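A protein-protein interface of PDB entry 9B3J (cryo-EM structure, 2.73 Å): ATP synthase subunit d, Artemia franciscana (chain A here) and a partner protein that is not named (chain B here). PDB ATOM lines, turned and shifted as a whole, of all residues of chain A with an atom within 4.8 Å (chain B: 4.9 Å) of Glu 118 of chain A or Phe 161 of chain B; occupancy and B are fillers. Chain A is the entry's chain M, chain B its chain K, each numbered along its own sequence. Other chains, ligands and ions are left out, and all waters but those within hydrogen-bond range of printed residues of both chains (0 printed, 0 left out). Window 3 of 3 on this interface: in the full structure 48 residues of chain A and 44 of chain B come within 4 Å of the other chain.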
ATOM      1  N   ASN A 114     -18.062   0.195  -5.060  1.00  0.00           N
ATOM      2  CA  ASN A 114     -16.955   0.877  -5.723  1.00  0.00           C
ATOM      3  C   ASN A 114     -16.424   0.071  -6.904  1.00  0.00           C
ATOM      4  O   ASN A 114     -16.160   0.631  -7.976  1.00  0.00           O
ATOM      5  CB  ASN A 114     -15.836   1.156  -4.724  1.00  0.00           C
ATOM      6  CG  ASN A 114     -16.246   2.148  -3.660  1.00  0.00           C
ATOM      7  OD1 ASN A 114     -17.070   3.028  -3.902  1.00  0.00           O
ATOM      8  ND2 ASN A 114     -15.675   2.009  -2.470  1.00  0.00           N
ATOM      9  N   TYR A 115     -16.272  -1.244  -6.729  1.00  0.00           N
ATOM     10  CA  TYR A 115     -15.759  -2.080  -7.807  1.00  0.00           C
ATOM     11  C   TYR A 115     -16.742  -2.164  -8.966  1.00  0.00           C
ATOM     12  O   TYR A 115     -16.332  -2.173 -10.130  1.00  0.00           O
ATOM     13  CB  TYR A 115     -15.432  -3.473  -7.277  1.00  0.00           C
ATOM     14  CG  TYR A 115     -14.233  -3.505  -6.362  1.00  0.00           C
ATOM     15  CD1 TYR A 115     -13.192  -2.600  -6.520  1.00  0.00           C
ATOM     16  CD2 TYR A 115     -14.140  -4.437  -5.336  1.00  0.00           C
ATOM     17  CE1 TYR A 115     -12.092  -2.626  -5.685  1.00  0.00           C
ATOM     18  CE2 TYR A 115     -13.047  -4.466  -4.493  1.00  0.00           C
ATOM     19  CZ  TYR A 115     -12.025  -3.561  -4.674  1.00  0.00           C
ATOM     20  OH  TYR A 115     -10.934  -3.589  -3.839  1.00  0.00           O
ATOM     21  N   LYS A 116     -18.042  -2.216  -8.669  1.00  0.00           N
ATOM     22  CA  LYS A 116     -19.045  -2.241  -9.729  1.00  0.00           C
ATOM     23  C   LYS A 116     -19.099  -0.914 -10.472  1.00  0.00           C
ATOM     24  O   LYS A 116     -19.304  -0.890 -11.694  1.00  0.00           O
ATOM     25  CB  LYS A 116     -20.417  -2.582  -9.152  1.00  0.00           C
ATOM     26  CG  LYS A 116     -20.595  -4.044  -8.805  1.00  0.00           C
ATOM     27  CD  LYS A 116     -22.030  -4.336  -8.416  1.00  0.00           C
ATOM     28  CE  LYS A 116     -22.234  -5.814  -8.146  1.00  0.00           C
ATOM     29  NZ  LYS A 116     -23.640  -6.121  -7.772  1.00  0.00           N
ATOM     30  N   ALA A 117     -18.919   0.201  -9.756  1.00  0.00           N
ATOM     31  CA  ALA A 117     -18.860   1.500 -10.417  1.00  0.00           C
ATOM     32  C   ALA A 117     -17.641   1.608 -11.324  1.00  0.00           C
ATOM     33  O   ALA A 117     -17.739   2.117 -12.448  1.00  0.00           O
ATOM     34  CB  ALA A 117     -18.852   2.615  -9.373  1.00  0.00           C
ATOM     35  N   GLU A 118     -16.486   1.125 -10.855  1.00  0.00           N
ATOM     36  CA  GLU A 118     -15.277   1.161 -11.673  1.00  0.00           C
ATOM     37  C   GLU A 118     -15.394   0.245 -12.885  1.00  0.00           C
ATOM     38  O   GLU A 118     -14.945   0.599 -13.982  1.00  0.00           O
ATOM     39  CB  GLU A 118     -14.063   0.777 -10.832  1.00  0.00           C
ATOM     40  CG  GLU A 118     -13.708   1.791  -9.768  1.00  0.00           C
ATOM     41  CD  GLU A 118     -12.591   1.311  -8.870  1.00  0.00           C
ATOM     42  OE1 GLU A 118     -11.623   0.723  -9.394  1.00  0.00           O
ATOM     43  OE2 GLU A 118     -12.684   1.508  -7.640  1.00  0.00           O
ATOM     44  N   LEU A 119     -15.992  -0.934 -12.706  1.00  0.00           N
ATOM     45  CA  LEU A 119     -16.188  -1.845 -13.827  1.00  0.00           C
ATOM     46  C   LEU A 119     -17.144  -1.254 -14.855  1.00  0.00           C
ATOM     47  O   LEU A 119     -16.919  -1.384 -16.064  1.00  0.00           O
ATOM     48  CB  LEU A 119     -16.710  -3.188 -13.320  1.00  0.00           C
ATOM     49  CG  LEU A 119     -16.062  -4.457 -13.873  1.00  0.00           C
ATOM     50  CD1 LEU A 119     -16.625  -5.668 -13.159  1.00  0.00           C
ATOM     51  CD2 LEU A 119     -16.263  -4.586 -15.373  1.00  0.00           C
ATOM     52  N   GLY A 120     -18.214  -0.604 -14.393  1.00  0.00           N
ATOM     53  CA  GLY A 120     -19.136   0.029 -15.322  1.00  0.00           C
ATOM     54  C   GLY A 120     -18.514   1.199 -16.056  1.00  0.00           C
ATOM     55  O   GLY A 120     -18.776   1.406 -17.244  1.00  0.00           O
ATOM     56  N   LYS A 121     -17.689   1.985 -15.358  1.00  0.00           N
ATOM     57  CA  LYS A 121     -17.016   3.109 -15.997  1.00  0.00           C
ATOM     58  C   LYS A 121     -16.032   2.634 -17.057  1.00  0.00           C
ATOM     59  O   LYS A 121     -15.963   3.214 -18.147  1.00  0.00           O
ATOM     60  CB  LYS A 121     -16.306   3.959 -14.947  1.00  0.00           C
ATOM     61  CG  LYS A 121     -15.708   5.237 -15.493  1.00  0.00           C
ATOM     62  CD  LYS A 121     -15.171   6.111 -14.375  1.00  0.00           C
ATOM     63  CE  LYS A 121     -14.663   7.438 -14.914  1.00  0.00           C
ATOM     64  NZ  LYS A 121     -14.174   8.335 -13.832  1.00  0.00           N
ATOM     65  N   LEU A 122     -15.276   1.571 -16.764  1.00  0.00           N
ATOM     66  CA  LEU A 122     -14.339   1.046 -17.753  1.00  0.00           C
ATOM     67  C   LEU A 122     -15.059   0.374 -18.913  1.00  0.00           C
ATOM     68  O   LEU A 122     -14.545   0.366 -20.037  1.00  0.00           O
ATOM     69  CB  LEU A 122     -13.370   0.063 -17.105  1.00  0.00           C
ATOM     70  CG  LEU A 122     -12.414   0.625 -16.055  1.00  0.00           C
ATOM     71  CD1 LEU A 122     -11.273  -0.348 -15.837  1.00  0.00           C
ATOM     72  CD2 LEU A 122     -11.888   1.993 -16.453  1.00  0.00           C
ATOM     73  N   SER B 157      -7.865  -5.404 -16.206  1.00  0.00           N
ATOM     74  CA  SER B 157      -8.653  -4.631 -15.249  1.00  0.00           C
ATOM     75  C   SER B 157     -10.027  -5.249 -15.025  1.00  0.00           C
ATOM     76  O   SER B 157     -10.527  -5.270 -13.888  1.00  0.00           O
ATOM     77  CB  SER B 157      -8.789  -3.189 -15.723  1.00  0.00           C
ATOM     78  OG  SER B 157      -7.551  -2.515 -15.622  1.00  0.00           O
ATOM     79  N   LYS B 158     -10.653  -5.761 -16.093  1.00  0.00           N
ATOM     80  CA  LYS B 158     -11.929  -6.460 -15.926  1.00  0.00           C
ATOM     81  C   LYS B 158     -11.774  -7.722 -15.080  1.00  0.00           C
ATOM     82  O   LYS B 158     -12.606  -8.003 -14.200  1.00  0.00           O
ATOM     83  CB  LYS B 158     -12.516  -6.813 -17.287  1.00  0.00           C
ATOM     84  CG  LYS B 158     -12.928  -5.620 -18.107  1.00  0.00           C
ATOM     85  CD  LYS B 158     -13.335  -6.053 -19.503  1.00  0.00           C
ATOM     86  CE  LYS B 158     -13.659  -4.856 -20.378  1.00  0.00           C
ATOM     87  NZ  LYS B 158     -13.934  -5.255 -21.785  1.00  0.00           N
ATOM     88  N   ILE B 159     -10.706  -8.488 -15.328  1.00  0.00           N
ATOM     89  CA  ILE B 159     -10.458  -9.712 -14.568  1.00  0.00           C
ATOM     90  C   ILE B 159     -10.188  -9.391 -13.103  1.00  0.00           C
ATOM     91  O   ILE B 159     -10.701 -10.065 -12.199  1.00  0.00           O
ATOM     92  CB  ILE B 159      -9.303 -10.502 -15.210  1.00  0.00           C
ATOM     93  CG1 ILE B 159      -9.746 -11.086 -16.551  1.00  0.00           C
ATOM     94  CG2 ILE B 159      -8.816 -11.610 -14.295  1.00  0.00           C
ATOM     95  CD1 ILE B 159      -8.647 -11.805 -17.294  1.00  0.00           C
ATOM     96  N   GLY B 160      -9.398  -8.346 -12.845  1.00  0.00           N
ATOM     97  CA  GLY B 160      -9.098  -7.970 -11.474  1.00  0.00           C
ATOM     98  C   GLY B 160     -10.317  -7.495 -10.708  1.00  0.00           C
ATOM     99  O   GLY B 160     -10.463  -7.786  -9.516  1.00  0.00           O
ATOM    100  N   PHE B 161     -11.224  -6.781 -11.384  1.00  0.00           N
ATOM    101  CA  PHE B 161     -12.450  -6.345 -10.717  1.00  0.00           C
ATOM    102  C   PHE B 161     -13.364  -7.523 -10.396  1.00  0.00           C
ATOM    103  O   PHE B 161     -13.968  -7.575  -9.311  1.00  0.00           O
ATOM    104  CB  PHE B 161     -13.182  -5.321 -11.579  1.00  0.00           C
ATOM    105  CG  PHE B 161     -12.514  -3.977 -11.621  1.00  0.00           C
ATOM    106  CD1 PHE B 161     -11.551  -3.633 -10.687  1.00  0.00           C
ATOM    107  CD2 PHE B 161     -12.855  -3.056 -12.593  1.00  0.00           C
ATOM    108  CE1 PHE B 161     -10.940  -2.398 -10.727  1.00  0.00           C
ATOM    109  CE2 PHE B 161     -12.247  -1.818 -12.636  1.00  0.00           C
ATOM    110  CZ  PHE B 161     -11.289  -1.491 -11.704  1.00  0.00           C
ATOM    111  N   GLU B 162     -13.477  -8.482 -11.322  1.00  0.00           N
ATOM    112  CA  GLU B 162     -14.314  -9.651 -11.057  1.00  0.00           C
ATOM    113  C   GLU B 162     -13.738 -10.518  -9.937  1.00  0.00           C
ATOM    114  O   GLU B 162     -14.486 -11.034  -9.090  1.00  0.00           O
ATOM    115  CB  GLU B 162     -14.484 -10.462 -12.337  1.00  0.00           C
ATOM    116  CG  GLU B 162     -15.231  -9.723 -13.428  1.00  0.00           C
ATOM    117  CD  GLU B 162     -14.975 -10.308 -14.800  1.00  0.00           C
ATOM    118  OE1 GLU B 162     -14.357 -11.389 -14.882  1.00  0.00           O
ATOM    119  OE2 GLU B 162     -15.388  -9.685 -15.799  1.00  0.00           O
ATOM    120  N   GLU B 163     -12.411 -10.682  -9.914  1.00  0.00           N
ATOM    121  CA  GLU B 163     -11.776 -11.442  -8.842  1.00  0.00           C
ATOM    122  C   GLU B 163     -11.939 -10.749  -7.497  1.00  0.00           C
ATOM    123  O   GLU B 163     -12.105 -11.416  -6.467  1.00  0.00           O
ATOM    124  CB  GLU B 163     -10.296 -11.658  -9.146  1.00  0.00           C
ATOM    125  CG  GLU B 163     -10.018 -12.682 -10.223  1.00  0.00           C
ATOM    126  CD  GLU B 163      -8.534 -12.882 -10.451  1.00  0.00           C
ATOM    127  OE1 GLU B 163      -7.734 -12.276  -9.707  1.00  0.00           O
ATOM    128  OE2 GLU B 163      -8.169 -13.639 -11.371  1.00  0.00           O
ATOM    129  N   ALA B 164     -11.886  -9.412  -7.483  1.00  0.00           N
ATOM    130  CA  ALA B 164     -12.104  -8.677  -6.241  1.00  0.00           C
ATOM    131  C   ALA B 164     -13.528  -8.863  -5.728  1.00  0.00           C
ATOM    132  O   ALA B 164     -13.751  -8.964  -4.511  1.00  0.00           O
ATOM    133  CB  ALA B 164     -11.795  -7.199  -6.452  1.00  0.00           C
ATOM    134  N   ILE B 165     -14.500  -8.919  -6.642  1.00  0.00           N
ATOM    135  CA  ILE B 165     -15.885  -9.162  -6.237  1.00  0.00           C
ATOM    136  C   ILE B 165     -16.035 -10.553  -5.619  1.00  0.00           C
ATOM    137  O   ILE B 165     -16.662 -10.722  -4.559  1.00  0.00           O
ATOM    138  CB  ILE B 165     -16.826  -8.965  -7.437  1.00  0.00           C
ATOM    139  CG1 ILE B 165     -16.876  -7.488  -7.813  1.00  0.00           C
ATOM    140  CG2 ILE B 165     -18.223  -9.472  -7.126  1.00  0.00           C
ATOM    141  CD1 ILE B 165     -17.340  -6.604  -6.684  1.00  0.00           C
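Along chain A the printed residues that touch a printed residue of chain B span positions 115 to 122.
Printed residues of chain B that touch a printed residue of chain A: Ser 157, Phe 161, Ala 164 and Ile 165.
Hydrophobic or aromatic side chains of chain B that line the printed part of chain A: Phe 161, Ala 164 and Ile 165.
Among the printed residues, 6 pairs touch across the chains.
Of the printed residues of chain B, Tyr 115 of chain A touches Ala 164 and Ile 165.
Ala 117 of chain A touches none of the printed residues of chain B.
Glu 118 of chain A touches just one residue of chain B: Phe 161 (3.2 Å).
Of the printed residues of chain B, Leu 119 of chain A touches Phe 161.
Printed residues of chain B within 4 Å of Leu 122 of chain A: Ser 157 and Phe 161.
Ile 159 of chain B touches none of the printed residues of chain A.
Phe 161 of chain B touches three residues of chain A.
The nearest residue of chain A that does not touch Phe 161 of chain B is Tyr 115 of chain A (4.4 Å).
CE2 of Tyr 115 of chain A touches CB of Ala 164 of chain B, 3.6 Å away.
Ile 165 of chain B touches Tyr 115 of chain A (CD1 to CB, 3.7 Å).
OE1 of Glu 118 of chain A touches CZ of Phe 161 of chain B (3.2 Å).
Leu 119 of chain A touches Phe 161 of chain B.
Leu 122 of chain A touches Ser 157 of chain B.
Phe 161 of chain B touches Leu 122 of chain A.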
